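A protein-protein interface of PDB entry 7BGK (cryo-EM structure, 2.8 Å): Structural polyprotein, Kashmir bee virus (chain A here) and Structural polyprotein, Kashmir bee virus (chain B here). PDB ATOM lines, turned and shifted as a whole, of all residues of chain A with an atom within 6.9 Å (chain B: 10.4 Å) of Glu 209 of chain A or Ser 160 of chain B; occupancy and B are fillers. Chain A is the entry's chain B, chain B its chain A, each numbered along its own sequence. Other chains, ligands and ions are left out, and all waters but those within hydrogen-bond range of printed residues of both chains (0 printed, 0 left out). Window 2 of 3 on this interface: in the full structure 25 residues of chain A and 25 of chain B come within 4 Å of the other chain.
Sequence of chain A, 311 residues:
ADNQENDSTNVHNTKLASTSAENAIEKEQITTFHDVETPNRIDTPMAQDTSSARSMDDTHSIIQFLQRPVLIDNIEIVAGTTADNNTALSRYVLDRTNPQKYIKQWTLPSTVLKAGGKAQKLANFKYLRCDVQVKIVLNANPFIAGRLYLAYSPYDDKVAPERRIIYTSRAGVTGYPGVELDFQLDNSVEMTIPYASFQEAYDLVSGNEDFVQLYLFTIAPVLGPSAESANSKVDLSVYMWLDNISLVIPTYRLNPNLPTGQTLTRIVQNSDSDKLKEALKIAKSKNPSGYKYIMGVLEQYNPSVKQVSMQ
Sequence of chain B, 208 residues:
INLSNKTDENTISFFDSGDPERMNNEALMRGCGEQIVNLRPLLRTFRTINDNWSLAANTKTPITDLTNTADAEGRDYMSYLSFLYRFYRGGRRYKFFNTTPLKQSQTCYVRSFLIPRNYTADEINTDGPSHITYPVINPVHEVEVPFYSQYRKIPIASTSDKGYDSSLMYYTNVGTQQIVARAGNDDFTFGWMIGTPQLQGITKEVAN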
ATOM      1  N   LEU A 108     -19.587  -2.124 -29.540  1.00  0.00           N
ATOM      2  CA  LEU A 108     -18.406  -2.098 -28.710  1.00  0.00           C
ATOM      3  C   LEU A 108     -18.119  -0.686 -28.223  1.00  0.00           C
ATOM      4  O   LEU A 108     -18.415   0.287 -28.921  1.00  0.00           O
ATOM      5  CB  LEU A 108     -17.189  -2.629 -29.470  1.00  0.00           C
ATOM      6  CG  LEU A 108     -17.281  -4.084 -29.907  1.00  0.00           C
ATOM      7  CD1 LEU A 108     -16.292  -4.353 -30.996  1.00  0.00           C
ATOM      8  CD2 LEU A 108     -17.042  -4.988 -28.738  1.00  0.00           C
ATOM      9  N   PRO A 109     -17.528  -0.541 -27.029  1.00  0.00           N
ATOM     10  CA  PRO A 109     -17.091  -1.633 -26.156  1.00  0.00           C
ATOM     11  C   PRO A 109     -18.165  -2.148 -25.196  1.00  0.00           C
ATOM     12  O   PRO A 109     -17.853  -2.990 -24.362  1.00  0.00           O
ATOM     13  CB  PRO A 109     -15.939  -1.001 -25.386  1.00  0.00           C
ATOM     14  CG  PRO A 109     -16.291   0.422 -25.304  1.00  0.00           C
ATOM     15  CD  PRO A 109     -17.072   0.766 -26.531  1.00  0.00           C
ATOM     16  N   SER A 110     -19.403  -1.665 -25.329  1.00  0.00           N
ATOM     17  CA  SER A 110     -20.461  -2.021 -24.385  1.00  0.00           C
ATOM     18  C   SER A 110     -20.543  -3.526 -24.169  1.00  0.00           C
ATOM     19  O   SER A 110     -20.560  -4.004 -23.030  1.00  0.00           O
ATOM     20  CB  SER A 110     -21.817  -1.519 -24.878  1.00  0.00           C
ATOM     21  OG  SER A 110     -21.946  -0.124 -25.043  1.00  0.00           O
ATOM     22  N   LYS A 158     -23.637   5.763 -36.082  1.00  0.00           N
ATOM     23  CA  LYS A 158     -23.721   7.212 -36.018  1.00  0.00           C
ATOM     24  C   LYS A 158     -23.298   7.906 -37.302  1.00  0.00           C
ATOM     25  O   LYS A 158     -23.499   9.118 -37.422  1.00  0.00           O
ATOM     26  CB  LYS A 158     -22.860   7.728 -34.859  1.00  0.00           C
ATOM     27  CG  LYS A 158     -23.309   7.236 -33.503  1.00  0.00           C
ATOM     28  CD  LYS A 158     -22.806   8.122 -32.390  1.00  0.00           C
ATOM     29  CE  LYS A 158     -21.331   7.893 -32.116  1.00  0.00           C
ATOM     30  NZ  LYS A 158     -21.082   6.545 -31.563  1.00  0.00           N
ATOM     31  N   SER A 197     -12.658   5.970 -29.834  1.00  0.00           N
ATOM     32  CA  SER A 197     -13.283   7.240 -29.520  1.00  0.00           C
ATOM     33  C   SER A 197     -12.468   8.399 -30.066  1.00  0.00           C
ATOM     34  O   SER A 197     -11.238   8.351 -30.141  1.00  0.00           O
ATOM     35  CB  SER A 197     -13.450   7.403 -28.016  1.00  0.00           C
ATOM     36  OG  SER A 197     -14.314   8.475 -27.719  1.00  0.00           O
ATOM     37  N   PHE A 198     -13.182   9.445 -30.465  1.00  0.00           N
ATOM     38  CA  PHE A 198     -12.570  10.691 -30.894  1.00  0.00           C
ATOM     39  C   PHE A 198     -12.193  11.579 -29.724  1.00  0.00           C
ATOM     40  O   PHE A 198     -11.510  12.588 -29.925  1.00  0.00           O
ATOM     41  CB  PHE A 198     -13.515  11.448 -31.822  1.00  0.00           C
ATOM     42  CG  PHE A 198     -14.787  11.893 -31.166  1.00  0.00           C
ATOM     43  CD1 PHE A 198     -15.838  11.019 -30.991  1.00  0.00           C
ATOM     44  CD2 PHE A 198     -14.937  13.194 -30.745  1.00  0.00           C
ATOM     45  CE1 PHE A 198     -16.995  11.431 -30.399  1.00  0.00           C
ATOM     46  CE2 PHE A 198     -16.096  13.606 -30.151  1.00  0.00           C
ATOM     47  CZ  PHE A 198     -17.124  12.725 -29.978  1.00  0.00           C
ATOM     48  N   GLN A 199     -12.612  11.222 -28.518  1.00  0.00           N
ATOM     49  CA  GLN A 199     -12.353  11.995 -27.320  1.00  0.00           C
ATOM     50  C   GLN A 199     -11.338  11.269 -26.452  1.00  0.00           C
ATOM     51  O   GLN A 199     -10.989  10.115 -26.695  1.00  0.00           O
ATOM     52  CB  GLN A 199     -13.656  12.266 -26.563  1.00  0.00           C
ATOM     53  CG  GLN A 199     -14.582  11.096 -26.390  1.00  0.00           C
ATOM     54  CD  GLN A 199     -15.969  11.521 -25.979  1.00  0.00           C
ATOM     55  OE1 GLN A 199     -16.266  12.709 -25.884  1.00  0.00           O
ATOM     56  NE2 GLN A 199     -16.829  10.549 -25.730  1.00  0.00           N
ATOM     57  N   TYR A 202     -13.169   7.064 -22.870  1.00  0.00           N
ATOM     58  CA  TYR A 202     -14.561   6.659 -22.765  1.00  0.00           C
ATOM     59  C   TYR A 202     -15.152   7.185 -21.466  1.00  0.00           C
ATOM     60  O   TYR A 202     -14.557   7.027 -20.400  1.00  0.00           O
ATOM     61  CB  TYR A 202     -14.680   5.137 -22.798  1.00  0.00           C
ATOM     62  CG  TYR A 202     -14.294   4.469 -24.091  1.00  0.00           C
ATOM     63  CD1 TYR A 202     -14.784   4.914 -25.301  1.00  0.00           C
ATOM     64  CD2 TYR A 202     -13.464   3.362 -24.095  1.00  0.00           C
ATOM     65  CE1 TYR A 202     -14.443   4.290 -26.473  1.00  0.00           C
ATOM     66  CE2 TYR A 202     -13.121   2.736 -25.262  1.00  0.00           C
ATOM     67  CZ  TYR A 202     -13.615   3.204 -26.449  1.00  0.00           C
ATOM     68  OH  TYR A 202     -13.274   2.579 -27.619  1.00  0.00           O
ATOM     69  N   ASP A 203     -16.323   7.808 -21.552  1.00  0.00           N
ATOM     70  CA  ASP A 203     -17.060   8.239 -20.369  1.00  0.00           C
ATOM     71  C   ASP A 203     -17.981   7.102 -19.940  1.00  0.00           C
ATOM     72  O   ASP A 203     -18.924   6.751 -20.656  1.00  0.00           O
ATOM     73  CB  ASP A 203     -17.838   9.518 -20.653  1.00  0.00           C
ATOM     74  CG  ASP A 203     -18.307  10.205 -19.392  1.00  0.00           C
ATOM     75  OD1 ASP A 203     -18.433   9.526 -18.355  1.00  0.00           O
ATOM     76  OD2 ASP A 203     -18.535  11.431 -19.432  1.00  0.00           O
ATOM     77  N   SER A 206     -21.691   9.274 -17.962  1.00  0.00           N
ATOM     78  CA  SER A 206     -22.596  10.126 -18.722  1.00  0.00           C
ATOM     79  C   SER A 206     -22.878   9.541 -20.098  1.00  0.00           C
ATOM     80  O   SER A 206     -24.022   9.207 -20.422  1.00  0.00           O
ATOM     81  CB  SER A 206     -21.988  11.524 -18.861  1.00  0.00           C
ATOM     82  OG  SER A 206     -22.816  12.374 -19.631  1.00  0.00           O
ATOM     83  N   GLY A 207     -21.844   9.411 -20.918  1.00  0.00           N
ATOM     84  CA  GLY A 207     -22.018   8.966 -22.279  1.00  0.00           C
ATOM     85  C   GLY A 207     -22.027   7.461 -22.420  1.00  0.00           C
ATOM     86  O   GLY A 207     -20.972   6.820 -22.371  1.00  0.00           O
ATOM     87  N   ASN A 208     -23.212   6.878 -22.582  1.00  0.00           N
ATOM     88  CA  ASN A 208     -23.322   5.466 -22.938  1.00  0.00           C
ATOM     89  C   ASN A 208     -23.300   5.341 -24.461  1.00  0.00           C
ATOM     90  O   ASN A 208     -24.257   4.922 -25.107  1.00  0.00           O
ATOM     91  CB  ASN A 208     -24.585   4.859 -22.336  1.00  0.00           C
ATOM     92  CG  ASN A 208     -24.652   3.354 -22.517  1.00  0.00           C
ATOM     93  OD1 ASN A 208     -23.834   2.765 -23.223  1.00  0.00           O
ATOM     94  ND2 ASN A 208     -25.625   2.726 -21.872  1.00  0.00           N
ATOM     95  N   GLU A 209     -22.160   5.726 -25.023  1.00  0.00           N
ATOM     96  CA  GLU A 209     -21.954   5.748 -26.460  1.00  0.00           C
ATOM     97  C   GLU A 209     -21.085   4.577 -26.888  1.00  0.00           C
ATOM     98  O   GLU A 209     -20.188   4.145 -26.162  1.00  0.00           O
ATOM     99  CB  GLU A 209     -21.281   7.053 -26.889  1.00  0.00           C
ATOM    100  CG  GLU A 209     -22.126   8.299 -26.736  1.00  0.00           C
ATOM    101  CD  GLU A 209     -21.317   9.567 -26.924  1.00  0.00           C
ATOM    102  OE1 GLU A 209     -20.086   9.469 -27.105  1.00  0.00           O
ATOM    103  OE2 GLU A 209     -21.909  10.663 -26.879  1.00  0.00           O
ATOM    104  N   ASP A 210     -21.368   4.064 -28.078  1.00  0.00           N
ATOM    105  CA  ASP A 210     -20.546   3.049 -28.710  1.00  0.00           C
ATOM    106  C   ASP A 210     -19.922   3.640 -29.963  1.00  0.00           C
ATOM    107  O   ASP A 210     -20.547   4.447 -30.656  1.00  0.00           O
ATOM    108  CB  ASP A 210     -21.367   1.811 -29.055  1.00  0.00           C
ATOM    109  CG  ASP A 210     -21.682   0.971 -27.840  1.00  0.00           C
ATOM    110  OD1 ASP A 210     -20.779   0.773 -27.003  1.00  0.00           O
ATOM    111  OD2 ASP A 210     -22.835   0.512 -27.714  1.00  0.00           O
ATOM    112  N   PHE A 211     -18.687   3.238 -30.248  1.00  0.00           N
ATOM    113  CA  PHE A 211     -17.896   3.887 -31.274  1.00  0.00           C
ATOM    114  C   PHE A 211     -17.401   2.952 -32.362  1.00  0.00           C
ATOM    115  O   PHE A 211     -16.875   3.436 -33.370  1.00  0.00           O
ATOM    116  CB  PHE A 211     -16.690   4.591 -30.639  1.00  0.00           C
ATOM    117  CG  PHE A 211     -17.053   5.547 -29.554  1.00  0.00           C
ATOM    118  CD1 PHE A 211     -17.370   6.855 -29.847  1.00  0.00           C
ATOM    119  CD2 PHE A 211     -17.086   5.140 -28.241  1.00  0.00           C
ATOM    120  CE1 PHE A 211     -17.704   7.730 -28.856  1.00  0.00           C
ATOM    121  CE2 PHE A 211     -17.423   6.016 -27.248  1.00  0.00           C
ATOM    122  CZ  PHE A 211     -17.732   7.312 -27.557  1.00  0.00           C
ATOM    123  N   ASN A 255     -23.430   3.839 -14.180  1.00  0.00           N
ATOM    124  CA  ASN A 255     -24.316   3.692 -15.324  1.00  0.00           C
ATOM    125  C   ASN A 255     -25.285   2.552 -15.045  1.00  0.00           C
ATOM    126  O   ASN A 255     -24.853   1.390 -14.992  1.00  0.00           O
ATOM    127  CB  ASN A 255     -23.521   3.413 -16.589  1.00  0.00           C
ATOM    128  CG  ASN A 255     -24.117   4.084 -17.806  1.00  0.00           C
ATOM    129  OD1 ASN A 255     -25.283   4.474 -17.806  1.00  0.00           O
ATOM    130  ND2 ASN A 255     -23.319   4.218 -18.852  1.00  0.00           N
ATOM    131  N   ARG B 117     -18.834  24.363 -35.438  1.00  0.00           N
ATOM    132  CA  ARG B 117     -19.523  23.559 -36.431  1.00  0.00           C
ATOM    133  C   ARG B 117     -20.915  23.191 -35.947  1.00  0.00           C
ATOM    134  O   ARG B 117     -21.139  22.958 -34.757  1.00  0.00           O
ATOM    135  CB  ARG B 117     -18.733  22.291 -36.737  1.00  0.00           C
ATOM    136  CG  ARG B 117     -17.945  22.355 -38.011  1.00  0.00           C
ATOM    137  CD  ARG B 117     -17.345  21.020 -38.369  1.00  0.00           C
ATOM    138  NE  ARG B 117     -18.346  20.069 -38.837  1.00  0.00           N
ATOM    139  CZ  ARG B 117     -18.636  18.911 -38.248  1.00  0.00           C
ATOM    140  NH1 ARG B 117     -18.009  18.529 -37.145  1.00  0.00           N
ATOM    141  NH2 ARG B 117     -19.567  18.128 -38.773  1.00  0.00           N
ATOM    142  N   ASN B 118     -21.856  23.146 -36.886  1.00  0.00           N
ATOM    143  CA  ASN B 118     -23.237  22.752 -36.653  1.00  0.00           C
ATOM    144  C   ASN B 118     -23.998  23.766 -35.813  1.00  0.00           C
ATOM    145  O   ASN B 118     -25.127  23.489 -35.393  1.00  0.00           O
ATOM    146  CB  ASN B 118     -23.308  21.372 -35.999  1.00  0.00           C
ATOM    147  CG  ASN B 118     -22.551  20.324 -36.783  1.00  0.00           C
ATOM    148  OD1 ASN B 118     -22.651  20.258 -38.007  1.00  0.00           O
ATOM    149  ND2 ASN B 118     -21.774  19.507 -36.084  1.00  0.00           N
ATOM    150  N   TYR B 119     -23.414  24.931 -35.556  1.00  0.00           N
ATOM    151  CA  TYR B 119     -24.140  26.035 -34.961  1.00  0.00           C
ATOM    152  C   TYR B 119     -24.915  26.794 -36.031  1.00  0.00           C
ATOM    153  O   TYR B 119     -24.705  26.620 -37.234  1.00  0.00           O
ATOM    154  CB  TYR B 119     -23.188  26.995 -34.254  1.00  0.00           C
ATOM    155  CG  TYR B 119     -22.897  26.680 -32.814  1.00  0.00           C
ATOM    156  CD1 TYR B 119     -22.799  25.376 -32.373  1.00  0.00           C
ATOM    157  CD2 TYR B 119     -22.690  27.693 -31.898  1.00  0.00           C
ATOM    158  CE1 TYR B 119     -22.521  25.091 -31.064  1.00  0.00           C
ATOM    159  CE2 TYR B 119     -22.411  27.417 -30.586  1.00  0.00           C
ATOM    160  CZ  TYR B 119     -22.326  26.114 -30.172  1.00  0.00           C
ATOM    161  OH  TYR B 119     -22.046  25.835 -28.859  1.00  0.00           O
ATOM    162  N   GLN B 150     -11.828  20.830 -29.322  1.00  0.00           N
ATOM    163  CA  GLN B 150     -11.688  20.169 -28.037  1.00  0.00           C
ATOM    164  C   GLN B 150     -11.125  18.764 -28.154  1.00  0.00           C
ATOM    165  O   GLN B 150     -10.794  18.159 -27.131  1.00  0.00           O
ATOM    166  CB  GLN B 150     -13.039  20.088 -27.330  1.00  0.00           C
ATOM    167  CG  GLN B 150     -13.680  21.404 -27.025  1.00  0.00           C
ATOM    168  CD  GLN B 150     -14.934  21.253 -26.211  1.00  0.00           C
ATOM    169  OE1 GLN B 150     -14.892  20.957 -25.020  1.00  0.00           O
ATOM    170  NE2 GLN B 150     -16.065  21.454 -26.849  1.00  0.00           N
ATOM    171  N   TYR B 151     -11.022  18.231 -29.368  1.00  0.00           N
ATOM    172  CA  TYR B 151     -10.603  16.861 -29.602  1.00  0.00           C
ATOM    173  C   TYR B 151      -9.488  16.836 -30.633  1.00  0.00           C
ATOM    174  O   TYR B 151      -9.407  17.702 -31.505  1.00  0.00           O
ATOM    175  CB  TYR B 151     -11.768  16.006 -30.081  1.00  0.00           C
ATOM    176  CG  TYR B 151     -12.999  16.123 -29.224  1.00  0.00           C
ATOM    177  CD1 TYR B 151     -13.089  15.463 -28.014  1.00  0.00           C
ATOM    178  CD2 TYR B 151     -14.069  16.897 -29.621  1.00  0.00           C
ATOM    179  CE1 TYR B 151     -14.203  15.572 -27.233  1.00  0.00           C
ATOM    180  CE2 TYR B 151     -15.189  17.008 -28.840  1.00  0.00           C
ATOM    181  CZ  TYR B 151     -15.251  16.342 -27.649  1.00  0.00           C
ATOM    182  OH  TYR B 151     -16.371  16.453 -26.868  1.00  0.00           O
ATOM    183  N   PRO B 155     -14.667  13.005 -35.863  1.00  0.00           N
ATOM    184  CA  PRO B 155     -15.265  11.953 -36.681  1.00  0.00           C
ATOM    185  C   PRO B 155     -16.183  12.533 -37.740  1.00  0.00           C
ATOM    186  O   PRO B 155     -16.891  13.517 -37.513  1.00  0.00           O
ATOM    187  CB  PRO B 155     -16.041  11.123 -35.658  1.00  0.00           C
ATOM    188  CG  PRO B 155     -16.440  12.087 -34.653  1.00  0.00           C
ATOM    189  CD  PRO B 155     -15.365  13.131 -34.573  1.00  0.00           C
ATOM    190  N   ALA B 157     -18.666  11.210 -38.514  1.00  0.00           N
ATOM    191  CA  ALA B 157     -19.983  10.805 -38.061  1.00  0.00           C
ATOM    192  C   ALA B 157     -20.654  11.912 -37.253  1.00  0.00           C
ATOM    193  O   ALA B 157     -20.121  13.010 -37.082  1.00  0.00           O
ATOM    194  CB  ALA B 157     -19.873   9.535 -37.227  1.00  0.00           C
ATOM    195  N   SER B 158     -21.846  11.610 -36.746  1.00  0.00           N
ATOM    196  CA  SER B 158     -22.553  12.505 -35.849  1.00  0.00           C
ATOM    197  C   SER B 158     -22.063  12.304 -34.417  1.00  0.00           C
ATOM    198  O   SER B 158     -21.395  11.321 -34.090  1.00  0.00           O
ATOM    199  CB  SER B 158     -24.058  12.279 -35.946  1.00  0.00           C
ATOM    200  OG  SER B 158     -24.423  11.018 -35.418  1.00  0.00           O
ATOM    201  N   THR B 159     -22.416  13.249 -33.551  1.00  0.00           N
ATOM    202  CA  THR B 159     -21.948  13.241 -32.175  1.00  0.00           C
ATOM    203  C   THR B 159     -23.036  13.750 -31.240  1.00  0.00           C
ATOM    204  O   THR B 159     -24.003  14.389 -31.660  1.00  0.00           O
ATOM    205  CB  THR B 159     -20.685  14.088 -32.020  1.00  0.00           C
ATOM    206  OG1 THR B 159     -20.925  15.396 -32.550  1.00  0.00           O
ATOM    207  CG2 THR B 159     -19.519  13.455 -32.743  1.00  0.00           C
ATOM    208  N   SER B 160     -22.861  13.452 -29.950  1.00  0.00           N
ATOM    209  CA  SER B 160     -23.679  14.082 -28.918  1.00  0.00           C
ATOM    210  C   SER B 160     -23.282  15.538 -28.720  1.00  0.00           C
ATOM    211  O   SER B 160     -24.142  16.422 -28.658  1.00  0.00           O
ATOM    212  CB  SER B 160     -23.539  13.317 -27.603  1.00  0.00           C
ATOM    213  OG  SER B 160     -23.769  11.935 -27.796  1.00  0.00           O
ATOM    214  N   ASP B 161     -21.982  15.806 -28.611  1.00  0.00           N
ATOM    215  CA  ASP B 161     -21.514  17.166 -28.406  1.00  0.00           C
ATOM    216  C   ASP B 161     -21.727  18.002 -29.661  1.00  0.00           C
ATOM    217  O   ASP B 161     -21.936  17.484 -30.760  1.00  0.00           O
ATOM    218  CB  ASP B 161     -20.037  17.165 -28.008  1.00  0.00           C
ATOM    219  CG  ASP B 161     -19.590  18.480 -27.401  1.00  0.00           C
ATOM    220  OD1 ASP B 161     -20.344  19.468 -27.492  1.00  0.00           O
ATOM    221  OD2 ASP B 161     -18.480  18.525 -26.831  1.00  0.00           O
ATOM    222  N   LYS B 162     -21.674  19.318 -29.479  1.00  0.00           N
ATOM    223  CA  LYS B 162     -21.848  20.256 -30.573  1.00  0.00           C
ATOM    224  C   LYS B 162     -20.964  21.464 -30.317  1.00  0.00           C
ATOM    225  O   LYS B 162     -20.684  21.815 -29.170  1.00  0.00           O
ATOM    226  CB  LYS B 162     -23.308  20.690 -30.725  1.00  0.00           C
ATOM    227  CG  LYS B 162     -23.625  21.275 -32.083  1.00  0.00           C
ATOM    228  CD  LYS B 162     -25.096  21.599 -32.230  1.00  0.00           C
ATOM    229  CE  LYS B 162     -25.475  22.819 -31.430  1.00  0.00           C
ATOM    230  NZ  LYS B 162     -26.842  23.286 -31.755  1.00  0.00           N
ATOM    231  N   GLY B 163     -20.526  22.093 -31.399  1.00  0.00           N
ATOM    232  CA  GLY B 163     -19.635  23.230 -31.293  1.00  0.00           C
ATOM    233  C   GLY B 163     -18.276  22.899 -30.722  1.00  0.00           C
ATOM    234  O   GLY B 163     -17.702  23.712 -29.987  1.00  0.00           O
ATOM    235  N   TYR B 164     -17.744  21.725 -31.043  1.00  0.00           N
ATOM    236  CA  TYR B 164     -16.459  21.282 -30.527  1.00  0.00           C
ATOM    237  C   TYR B 164     -15.311  21.559 -31.483  1.00  0.00           C
ATOM    238  O   TYR B 164     -14.161  21.283 -31.141  1.00  0.00           O
ATOM    239  CB  TYR B 164     -16.505  19.790 -30.191  1.00  0.00           C
ATOM    240  CG  TYR B 164     -17.062  18.906 -31.272  1.00  0.00           C
ATOM    241  CD1 TYR B 164     -18.394  18.551 -31.273  1.00  0.00           C
ATOM    242  CD2 TYR B 164     -16.251  18.401 -32.271  1.00  0.00           C
ATOM    243  CE1 TYR B 164     -18.909  17.741 -32.246  1.00  0.00           C
ATOM    244  CE2 TYR B 164     -16.761  17.586 -33.251  1.00  0.00           C
ATOM    245  CZ  TYR B 164     -18.091  17.257 -33.233  1.00  0.00           C
ATOM    246  OH  TYR B 164     -18.611  16.441 -34.210  1.00  0.00           O
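OG of Ser 160 of chain B sits at hydrogen-bond distance from OE2 of Glu 209 of chain A.
O of Lys 158 of chain A is in hydrogen-bond range of OG of Ser 158 of chain B (2.9 Å).
The side-chain carboxylate (OD2) of Asp 161 of chain B is in hydrogen-bond range of the side-chain hydroxyl (OH) of Tyr 151 of chain B (3.0 Å).
The side-chain hydroxyl of Thr 159 of chain B sits at hydrogen-bond distance from the side-chain hydroxyl of Tyr 164 of chain B, 3.0 Å away.
The side-chain hydroxyl of Thr 159 of chain B is in hydrogen-bond range of the backbone carbonyl oxygen of Asp 161 of chain B (2.9 Å).
OG of Ser 197 of chain A lies close to N of Gln 199 of chain A, at 3.3 Å.
Ala 157 of chain B touches Lys 158 of chain A.
Phe 198 of chain A touches Tyr 151 of chain B.
CD of Pro 155 of chain B touches CG of Phe 198 of chain A, 3.7 Å away.
Phe 198 of chain A touches Thr 159 of chain B (CZ to CG2, 3.7 Å).
Tyr 151 of chain B touches Gln 199 of chain A (CE1 to CB, 3.4 Å).
Ser 160 of chain B touches just one residue of chain A: Glu 209.
No residue of chain B comes within 4 Å of Gly 207 of chain A.
No residue of chain B comes within 4 Å of Asn 208 of chain A.
No residue of chain B comes within 4 Å of Asp 210 of chain A.
Of the printed residues of chain A, Thr 159 of chain B touches Phe 198.
Of the printed residues of chain A, Ala 157 of chain B touches Lys 158 (3.7 Å).
Printed residues of chain A within 4 Å of Pro 155 of chain B: Phe 198.
The nearest residue of chain B that does not touch Glu 209 of chain A is Asp 161 of chain B (5.4 Å).
The nearest residue of chain A that does not touch Ser 160 of chain B is Phe 198 of chain A (5.8 Å).
Of the 14 printed residues of chain B, 6 touch a printed residue of chain A.
Hydrophobic or aromatic side chains of chain B that line the printed part of chain A: Tyr 151, Pro 155 and Ala 157.
Among the printed residues, no Asp or Glu carboxylate lies within 4 Å of a Lys or Arg side-chain nitrogen of the other chain.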
